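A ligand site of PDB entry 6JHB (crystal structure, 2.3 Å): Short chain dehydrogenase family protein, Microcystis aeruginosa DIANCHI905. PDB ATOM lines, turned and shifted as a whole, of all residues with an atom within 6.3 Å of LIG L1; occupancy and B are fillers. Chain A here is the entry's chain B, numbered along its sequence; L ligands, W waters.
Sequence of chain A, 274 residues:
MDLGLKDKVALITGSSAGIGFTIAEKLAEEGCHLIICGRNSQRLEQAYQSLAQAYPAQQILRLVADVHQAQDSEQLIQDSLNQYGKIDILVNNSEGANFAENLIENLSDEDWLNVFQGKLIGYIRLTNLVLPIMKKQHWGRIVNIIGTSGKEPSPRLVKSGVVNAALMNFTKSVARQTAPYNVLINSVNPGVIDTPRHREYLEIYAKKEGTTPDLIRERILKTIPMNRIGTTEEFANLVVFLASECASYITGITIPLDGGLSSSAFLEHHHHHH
The side-chain hydroxyl (OG) of Ser 149 sits at hydrogen-bond distance from an oxygen (O3) of LIG L1 (2.7 Å). O1 of LIG L1 sits at hydrogen-bond distance from ND2 of Asn 164, at 3.0 Å. An oxygen (O1) of LIG L1 sits close to the side-chain hydroxyl (OG) of Ser 160 (3.2 Å). N of Thr 148 sits at hydrogen-bond distance from O4 of LIG L1 (3.0 Å). The side-chain amino group (NZ) of Lys 119 is in hydrogen-bond range of an oxygen (O12) of LG2 L2. O2 of LG2 L2 sits at hydrogen-bond distance from N of Arg 197, at 3.0 Å. An oxygen (O9) of LG2 L2 sits at hydrogen-bond distance from the side-chain hydroxyl (OG1) of Thr 195 (2.6 Å). The backbone NH of Ile 193 sits at hydrogen-bond distance from an oxygen (O14) of LG2 L2 (3.0 Å). N7 of LG2 L2 sits at hydrogen-bond distance from O of Ile 193.
OG of Ser 149 is in hydrogen-bond range of ND2 of Asn 164, 2.8 Å away. The side-chain hydroxyl (OG) of Ser 149 lies close to the backbone NH (N) of Gly 161, at 3.3 Å. The side-chain amide nitrogen (ND2) of Asn 164 sits close to the backbone carbonyl oxygen (O) of Gly 147. O of Ser 160 sits close to OD1 of Asn 164 (3.3 Å). O of Ile 146 sits at hydrogen-bond distance from NZ of Lys 119 (2.8 Å). The backbone NH (N) of His 198 lies within hydrogen-bond range of the side-chain hydroxyl (OG1) of Thr 195, 3.2 Å away. The guanidinium group (NH2) of Arg 197 lies within hydrogen-bond range of the backbone carbonyl oxygen (O) of Ala 97 (3.5 Å).
O1 of LIG L1 lies close to O of Ile 146. Merely in contact with LIG L1: Lys 119 (3.9 Å), Gly 147 (2.8 Å), Leu 157 (3.2 Å), Arg 197 (3.9 Å) and His 198 (3.7 Å). Hydrophobic or aromatic side chains within 4 Å of LIG L1: Leu 157 and His 198. Within 4 Å of LIG L1: Lys 119, Ile 146, Gly 147, Thr 148, Ser 149, Leu 157, Ser 160, Asn 164, Arg 197 and His 198. The nearest printed residue that does not touch LIG L1 is Phe 99 (4.1 Å).
Water W2 lies within hydrogen-bond range of OG1 of Thr 148 (2.6 Å), O4 of LIG L1 (2.9 Å), O of Gly 191 (2.9 Å) and O of Pro 190 (3.0 Å). Water W1 lies within hydrogen-bond range of OD1 of Asn 164 (3.0 Å), OG of Ser 160 (3.1 Å), NZ of Lys 119 (3.2 Å) and O1 of LIG L1 (3.3 Å).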
ATOM      1  N   GLY A  96     -28.411  16.682 -18.982  1.00  0.00           N
ATOM      2  CA  GLY A  96     -28.387  18.052 -18.495  1.00  0.00           C
ATOM      3  C   GLY A  96     -29.809  18.561 -18.584  1.00  0.00           C
ATOM      4  O   GLY A  96     -30.759  17.793 -18.735  1.00  0.00           O
ATOM      5  N   ALA A  97     -29.931  19.882 -18.542  1.00  0.00           N
ATOM      6  CA  ALA A  97     -31.194  20.542 -18.368  1.00  0.00           C
ATOM      7  C   ALA A  97     -32.034  20.408 -19.611  1.00  0.00           C
ATOM      8  O   ALA A  97     -31.509  20.226 -20.704  1.00  0.00           O
ATOM      9  CB  ALA A  97     -30.965  22.018 -18.026  1.00  0.00           C
ATOM     10  N   PHE A  99     -34.956  21.200 -22.660  1.00  0.00           N
ATOM     11  CA  PHE A  99     -34.983  22.189 -23.760  1.00  0.00           C
ATOM     12  C   PHE A  99     -36.280  23.007 -23.821  1.00  0.00           C
ATOM     13  O   PHE A  99     -36.503  23.724 -24.800  1.00  0.00           O
ATOM     14  CB  PHE A  99     -34.822  21.525 -25.135  1.00  0.00           C
ATOM     15  CG  PHE A  99     -33.672  20.564 -25.240  1.00  0.00           C
ATOM     16  CD1 PHE A  99     -32.444  20.815 -24.635  1.00  0.00           C
ATOM     17  CD2 PHE A  99     -33.816  19.406 -25.992  1.00  0.00           C
ATOM     18  CE1 PHE A  99     -31.395  19.914 -24.754  1.00  0.00           C
ATOM     19  CE2 PHE A  99     -32.767  18.505 -26.110  1.00  0.00           C
ATOM     20  CZ  PHE A  99     -31.559  18.757 -25.495  1.00  0.00           C
ATOM     21  N   LYS A 119     -27.407  17.050 -13.284  1.00  0.00           N
ATOM     22  CA  LYS A 119     -26.043  16.833 -13.776  1.00  0.00           C
ATOM     23  C   LYS A 119     -24.996  17.566 -12.963  1.00  0.00           C
ATOM     24  O   LYS A 119     -23.896  17.074 -12.803  1.00  0.00           O
ATOM     25  CB  LYS A 119     -25.969  17.260 -15.251  1.00  0.00           C
ATOM     26  CG  LYS A 119     -24.571  17.340 -15.885  1.00  0.00           C
ATOM     27  CD  LYS A 119     -24.751  17.620 -17.374  1.00  0.00           C
ATOM     28  CE  LYS A 119     -23.456  17.867 -18.104  1.00  0.00           C
ATOM     29  NZ  LYS A 119     -23.729  18.020 -19.561  1.00  0.00           N
ATOM     30  N   ILE A 146     -19.357  17.556 -20.747  1.00  0.00           N
ATOM     31  CA  ILE A 146     -20.020  18.788 -20.348  1.00  0.00           C
ATOM     32  C   ILE A 146     -20.899  19.355 -21.451  1.00  0.00           C
ATOM     33  O   ILE A 146     -22.023  18.918 -21.601  1.00  0.00           O
ATOM     34  CB  ILE A 146     -18.982  19.777 -19.811  1.00  0.00           C
ATOM     35  CG1 ILE A 146     -18.336  19.154 -18.583  1.00  0.00           C
ATOM     36  CG2 ILE A 146     -19.587  21.138 -19.480  1.00  0.00           C
ATOM     37  CD1 ILE A 146     -17.410  20.096 -17.846  1.00  0.00           C
ATOM     38  N   GLY A 147     -20.368  20.273 -22.249  1.00  0.00           N
ATOM     39  CA  GLY A 147     -21.125  21.013 -23.244  1.00  0.00           C
ATOM     40  C   GLY A 147     -20.529  22.390 -23.514  1.00  0.00           C
ATOM     41  O   GLY A 147     -20.101  23.076 -22.595  1.00  0.00           O
ATOM     42  N   THR A 148     -20.531  22.802 -24.778  1.00  0.00           N
ATOM     43  CA  THR A 148     -19.913  24.080 -25.192  1.00  0.00           C
ATOM     44  C   THR A 148     -20.630  25.315 -24.673  1.00  0.00           C
ATOM     45  O   THR A 148     -20.014  26.374 -24.498  1.00  0.00           O
ATOM     46  CB  THR A 148     -19.791  24.181 -26.723  1.00  0.00           C
ATOM     47  OG1 THR A 148     -21.050  23.891 -27.337  1.00  0.00           O
ATOM     48  CG2 THR A 148     -18.761  23.213 -27.237  1.00  0.00           C
ATOM     49  N   SER A 149     -21.913  25.172 -24.365  1.00  0.00           N
ATOM     50  CA  SER A 149     -22.692  26.211 -23.678  1.00  0.00           C
ATOM     51  C   SER A 149     -22.002  26.748 -22.429  1.00  0.00           C
ATOM     52  O   SER A 149     -22.235  27.891 -22.006  1.00  0.00           O
ATOM     53  CB  SER A 149     -24.074  25.679 -23.289  1.00  0.00           C
ATOM     54  OG  SER A 149     -24.011  24.731 -22.237  1.00  0.00           O
ATOM     55  N   GLY A 150     -21.149  25.911 -21.832  1.00  0.00           N
ATOM     56  CA  GLY A 150     -20.354  26.285 -20.675  1.00  0.00           C
ATOM     57  C   GLY A 150     -19.386  27.413 -20.966  1.00  0.00           C
ATOM     58  O   GLY A 150     -19.181  28.266 -20.133  1.00  0.00           O
ATOM     59  N   LEU A 157     -30.169  27.402 -24.134  1.00  0.00           N
ATOM     60  CA  LEU A 157     -29.273  26.719 -23.175  1.00  0.00           C
ATOM     61  C   LEU A 157     -28.836  27.537 -21.979  1.00  0.00           C
ATOM     62  O   LEU A 157     -27.668  27.495 -21.579  1.00  0.00           O
ATOM     63  CB  LEU A 157     -27.995  26.289 -23.886  1.00  0.00           C
ATOM     64  CG  LEU A 157     -28.054  25.321 -25.040  1.00  0.00           C
ATOM     65  CD1 LEU A 157     -26.739  25.389 -25.819  1.00  0.00           C
ATOM     66  CD2 LEU A 157     -28.290  23.913 -24.520  1.00  0.00           C
ATOM     67  N   SER A 160     -28.380  24.998 -18.925  1.00  0.00           N
ATOM     68  CA  SER A 160     -27.338  24.115 -19.344  1.00  0.00           C
ATOM     69  C   SER A 160     -26.009  24.803 -19.333  1.00  0.00           C
ATOM     70  O   SER A 160     -25.025  24.264 -18.865  1.00  0.00           O
ATOM     71  CB  SER A 160     -27.680  23.723 -20.764  1.00  0.00           C
ATOM     72  OG  SER A 160     -27.044  22.523 -21.063  1.00  0.00           O
ATOM     73  N   GLY A 161     -25.968  26.016 -19.878  1.00  0.00           N
ATOM     74  CA  GLY A 161     -24.728  26.789 -19.915  1.00  0.00           C
ATOM     75  C   GLY A 161     -24.233  27.150 -18.520  1.00  0.00           C
ATOM     76  O   GLY A 161     -23.025  27.240 -18.271  1.00  0.00           O
ATOM     77  N   ASN A 164     -22.789  24.022 -17.053  1.00  0.00           N
ATOM     78  CA  ASN A 164     -21.566  23.665 -17.717  1.00  0.00           C
ATOM     79  C   ASN A 164     -20.393  24.539 -17.322  1.00  0.00           C
ATOM     80  O   ASN A 164     -19.282  24.035 -17.094  1.00  0.00           O
ATOM     81  CB  ASN A 164     -21.791  23.674 -19.222  1.00  0.00           C
ATOM     82  CG  ASN A 164     -22.615  22.508 -19.689  1.00  0.00           C
ATOM     83  OD1 ASN A 164     -22.976  21.617 -18.895  1.00  0.00           O
ATOM     84  ND2 ASN A 164     -22.919  22.504 -20.968  1.00  0.00           N
ATOM     85  N   PRO A 190     -18.759  18.532 -26.007  1.00  0.00           N
ATOM     86  CA  PRO A 190     -19.267  18.256 -27.335  1.00  0.00           C
ATOM     87  C   PRO A 190     -19.944  19.476 -27.916  1.00  0.00           C
ATOM     88  O   PRO A 190     -20.618  20.194 -27.188  1.00  0.00           O
ATOM     89  CB  PRO A 190     -20.318  17.181 -27.088  1.00  0.00           C
ATOM     90  CG  PRO A 190     -20.723  17.349 -25.665  1.00  0.00           C
ATOM     91  CD  PRO A 190     -19.562  17.916 -24.934  1.00  0.00           C
ATOM     92  N   GLY A 191     -19.702  19.721 -29.200  1.00  0.00           N
ATOM     93  CA  GLY A 191     -20.455  20.695 -29.959  1.00  0.00           C
ATOM     94  C   GLY A 191     -21.785  20.070 -30.319  1.00  0.00           C
ATOM     95  O   GLY A 191     -22.744  20.135 -29.533  1.00  0.00           O
ATOM     96  N   ILE A 193     -23.120  16.415 -31.756  1.00  0.00           N
ATOM     97  CA  ILE A 193     -22.758  15.032 -31.953  1.00  0.00           C
ATOM     98  C   ILE A 193     -24.043  14.239 -32.104  1.00  0.00           C
ATOM     99  O   ILE A 193     -24.938  14.358 -31.296  1.00  0.00           O
ATOM    100  CB  ILE A 193     -22.017  14.483 -30.721  1.00  0.00           C
ATOM    101  CG1 ILE A 193     -20.773  15.326 -30.409  1.00  0.00           C
ATOM    102  CG2 ILE A 193     -21.697  13.016 -30.917  1.00  0.00           C
ATOM    103  CD1 ILE A 193     -19.826  15.513 -31.573  1.00  0.00           C
ATOM    104  N   THR A 195     -26.496  12.012 -31.565  1.00  0.00           N
ATOM    105  CA  THR A 195     -27.079  11.064 -30.585  1.00  0.00           C
ATOM    106  C   THR A 195     -28.610  11.104 -30.572  1.00  0.00           C
ATOM    107  O   THR A 195     -29.198  12.025 -31.132  1.00  0.00           O
ATOM    108  CB  THR A 195     -26.678  11.450 -29.168  1.00  0.00           C
ATOM    109  OG1 THR A 195     -27.128  12.778 -28.925  1.00  0.00           O
ATOM    110  CG2 THR A 195     -25.212  11.397 -28.990  1.00  0.00           C
ATOM    111  N   ARG A 197     -30.543  12.037 -27.959  1.00  0.00           N
ATOM    112  CA  ARG A 197     -30.840  13.369 -27.417  1.00  0.00           C
ATOM    113  C   ARG A 197     -30.752  14.532 -28.433  1.00  0.00           C
ATOM    114  O   ARG A 197     -31.536  15.507 -28.364  1.00  0.00           O
ATOM    115  CB  ARG A 197     -29.915  13.636 -26.258  1.00  0.00           C
ATOM    116  CG  ARG A 197     -30.196  14.925 -25.483  1.00  0.00           C
ATOM    117  CD  ARG A 197     -31.388  14.772 -24.554  1.00  0.00           C
ATOM    118  NE  ARG A 197     -31.503  15.898 -23.612  1.00  0.00           N
ATOM    119  CZ  ARG A 197     -32.636  16.319 -23.066  1.00  0.00           C
ATOM    120  NH1 ARG A 197     -33.784  15.709 -23.311  1.00  0.00           N
ATOM    121  NH2 ARG A 197     -32.634  17.348 -22.242  1.00  0.00           N
ATOM    122  N   HIS A 198     -29.805  14.458 -29.365  1.00  0.00           N
ATOM    123  CA  HIS A 198     -29.684  15.471 -30.416  1.00  0.00           C
ATOM    124  C   HIS A 198     -30.825  15.327 -31.407  1.00  0.00           C
ATOM    125  O   HIS A 198     -31.447  16.309 -31.778  1.00  0.00           O
ATOM    126  CB  HIS A 198     -28.340  15.378 -31.114  1.00  0.00           C
ATOM    127  CG  HIS A 198     -28.315  15.890 -32.515  1.00  0.00           C
ATOM    128  ND1 HIS A 198     -28.074  17.216 -32.821  1.00  0.00           N
ATOM    129  CD2 HIS A 198     -28.475  15.248 -33.703  1.00  0.00           C
ATOM    130  CE1 HIS A 198     -28.105  17.363 -34.128  1.00  0.00           C
ATOM    131  NE2 HIS A 198     -28.332  16.191 -34.691  1.00  0.00           N
ATOM    132  N   ARG A 199     -31.107  14.100 -31.823  1.00  0.00           N
ATOM    133  CA  ARG A 199     -32.251  13.864 -32.710  1.00  0.00           C
ATOM    134  C   ARG A 199     -33.578  14.259 -32.042  1.00  0.00           C
ATOM    135  O   ARG A 199     -34.487  14.766 -32.701  1.00  0.00           O
ATOM    136  CB  ARG A 199     -32.291  12.414 -33.213  1.00  0.00           C
ATOM    137  CG  ARG A 199     -31.539  12.194 -34.524  1.00  0.00           C
ATOM    138  CD  ARG A 199     -31.304  10.728 -34.861  1.00  0.00           C
ATOM    139  NE  ARG A 199     -29.934  10.330 -34.541  1.00  0.00           N
ATOM    140  CZ  ARG A 199     -29.536   9.397 -33.670  1.00  0.00           C
ATOM    141  NH1 ARG A 199     -30.403   8.663 -32.960  1.00  0.00           N
ATOM    142  NH2 ARG A 199     -28.235   9.188 -33.508  1.00  0.00           N
ATOM    143  N   TYR A 201     -33.787  16.571 -29.746  1.00  0.00           N
ATOM    144  CA  TYR A 201     -33.663  18.014 -29.763  1.00  0.00           C
ATOM    145  C   TYR A 201     -34.086  18.592 -31.123  1.00  0.00           C
ATOM    146  O   TYR A 201     -34.747  19.626 -31.188  1.00  0.00           O
ATOM    147  CB  TYR A 201     -32.229  18.372 -29.397  1.00  0.00           C
ATOM    148  CG  TYR A 201     -31.768  19.768 -29.739  1.00  0.00           C
ATOM    149  CD1 TYR A 201     -31.607  20.733 -28.745  1.00  0.00           C
ATOM    150  CD2 TYR A 201     -31.448  20.103 -31.060  1.00  0.00           C
ATOM    151  CE1 TYR A 201     -31.155  22.000 -29.061  1.00  0.00           C
ATOM    152  CE2 TYR A 201     -31.000  21.365 -31.383  1.00  0.00           C
ATOM    153  CZ  TYR A 201     -30.851  22.309 -30.382  1.00  0.00           C
ATOM    154  OH  TYR A 201     -30.406  23.578 -30.721  1.00  0.00           O
HETATM  155  O1  LIG L   1     -24.781  20.564 -22.279  1.00  0.00           O
HETATM  156  C1  LIG L   1     -27.260  20.550 -25.962  1.00  0.00           C
HETATM  157  C2  LIG L   1     -27.600  19.768 -27.063  1.00  0.00           C
HETATM  158  C3  LIG L   1     -27.726  18.399 -26.909  1.00  0.00           C
HETATM  159  C4  LIG L   1     -27.543  17.798 -25.668  1.00  0.00           C
HETATM  160  C5  LIG L   1     -27.206  18.581 -24.554  1.00  0.00           C
HETATM  161  C6  LIG L   1     -27.050  19.958 -24.716  1.00  0.00           C
HETATM  162  O2  LIG L   1     -28.050  17.662 -27.983  1.00  0.00           O
HETATM  163  C7  LIG L   1     -26.728  20.841 -23.529  1.00  0.00           C
HETATM  164  C8  LIG L   1     -25.274  21.129 -23.245  1.00  0.00           C
HETATM  165  C9  LIG L   1     -24.544  22.149 -24.036  1.00  0.00           C
HETATM  166  O3  LIG L   1     -25.079  23.250 -24.163  1.00  0.00           O
HETATM  167  O4  LIG L   1     -23.434  21.983 -24.570  1.00  0.00           O
HETATM  168  P1  LG2 L   2     -28.378  10.709 -25.034  1.00  0.00           P
HETATM  169  O1  LG2 L   2     -29.660  10.977 -24.342  1.00  0.00           O
HETATM  170  O2  LG2 L   2     -28.388  10.436 -26.529  1.00  0.00           O
HETATM  171  O3  LG2 L   2     -27.635   9.535 -24.226  1.00  0.00           O
HETATM  172  C1  LG2 L   2     -27.764   9.654 -22.814  1.00  0.00           C
HETATM  173  C2  LG2 L   2     -27.500   8.336 -22.138  1.00  0.00           C
HETATM  174  O4  LG2 L   2     -27.285   8.548 -20.739  1.00  0.00           O
HETATM  175  C3  LG2 L   2     -28.665   7.383 -22.218  1.00  0.00           C
HETATM  176  O5  LG2 L   2     -28.095   6.057 -22.169  1.00  0.00           O
HETATM  177  C4  LG2 L   2     -29.443   7.632 -20.966  1.00  0.00           C
HETATM  178  O6  LG2 L   2     -30.225   6.499 -20.601  1.00  0.00           O
HETATM  179  C5  LG2 L   2     -28.313   7.895 -19.983  1.00  0.00           C
HETATM  180  N1  LG2 L   2     -28.647   8.805 -18.880  1.00  0.00           N
HETATM  181  C6  LG2 L   2     -29.102  10.063 -18.986  1.00  0.00           C
HETATM  182  N2  LG2 L   2     -29.257  10.593 -17.748  1.00  0.00           N
HETATM  183  C7  LG2 L   2     -28.930   9.653 -16.846  1.00  0.00           C
HETATM  184  C8  LG2 L   2     -28.881   9.538 -15.373  1.00  0.00           C
HETATM  185  N3  LG2 L   2     -29.240  10.545 -14.562  1.00  0.00           N
HETATM  186  N4  LG2 L   2     -28.460   8.377 -14.849  1.00  0.00           N
HETATM  187  C9  LG2 L   2     -28.075   7.346 -15.631  1.00  0.00           C
HETATM  188  N5  LG2 L   2     -28.129   7.377 -16.966  1.00  0.00           N
HETATM  189  C10 LG2 L   2     -28.511   8.485 -17.607  1.00  0.00           C
HETATM  190  O7  LG2 L   2     -27.447  11.950 -24.597  1.00  0.00           O
HETATM  191  P2  LG2 L   2     -26.074  12.396 -25.333  1.00  0.00           P
HETATM  192  O8  LG2 L   2     -25.232  11.154 -25.557  1.00  0.00           O
HETATM  193  O9  LG2 L   2     -26.422  13.342 -26.493  1.00  0.00           O
HETATM  194  O10 LG2 L   2     -25.446  13.358 -24.194  1.00  0.00           O
HETATM  195  C11 LG2 L   2     -24.329  12.945 -23.394  1.00  0.00           C
HETATM  196  C12 LG2 L   2     -23.780  14.109 -22.576  1.00  0.00           C
HETATM  197  O11 LG2 L   2     -23.172  15.117 -23.398  1.00  0.00           O
HETATM  198  C13 LG2 L   2     -24.858  14.822 -21.769  1.00  0.00           C
HETATM  199  O12 LG2 L   2     -24.276  15.246 -20.530  1.00  0.00           O
HETATM  200  C14 LG2 L   2     -25.213  16.027 -22.610  1.00  0.00           C
HETATM  201  O13 LG2 L   2     -25.729  17.122 -21.840  1.00  0.00           O
HETATM  202  C15 LG2 L   2     -23.851  16.366 -23.229  1.00  0.00           C
HETATM  203  N6  LG2 L   2     -23.991  17.087 -24.482  1.00  0.00           N
HETATM  204  C16 LG2 L   2     -24.274  16.443 -25.615  1.00  0.00           C
HETATM  205  C17 LG2 L   2     -24.402  17.132 -26.826  1.00  0.00           C
HETATM  206  C18 LG2 L   2     -24.700  16.413 -28.099  1.00  0.00           C
HETATM  207  O14 LG2 L   2     -24.476  17.002 -29.156  1.00  0.00           O
HETATM  208  N7  LG2 L   2     -25.212  15.189 -28.032  1.00  0.00           N
HETATM  209  C19 LG2 L   2     -24.223  18.619 -26.930  1.00  0.00           C
HETATM  210  C20 LG2 L   2     -23.927  19.177 -25.626  1.00  0.00           C
HETATM  211  C21 LG2 L   2     -23.821  18.420 -24.463  1.00  0.00           C
HETATM  212  P3  LG2 L   2     -31.563   6.624 -19.702  1.00  0.00           P
HETATM  213  O15 LG2 L   2     -32.313   7.833 -20.210  1.00  0.00           O
HETATM  214  O16 LG2 L   2     -32.332   5.311 -19.859  1.00  0.00           O
HETATM  215  O17 LG2 L   2     -30.871   6.760 -18.366  1.00  0.00           O
HETATM  216  O   HOH W   1     -25.727  20.489 -19.131  1.00  0.00           O
HETATM  217  O   HOH W   2     -22.916  22.107 -27.410  1.00  0.00           O
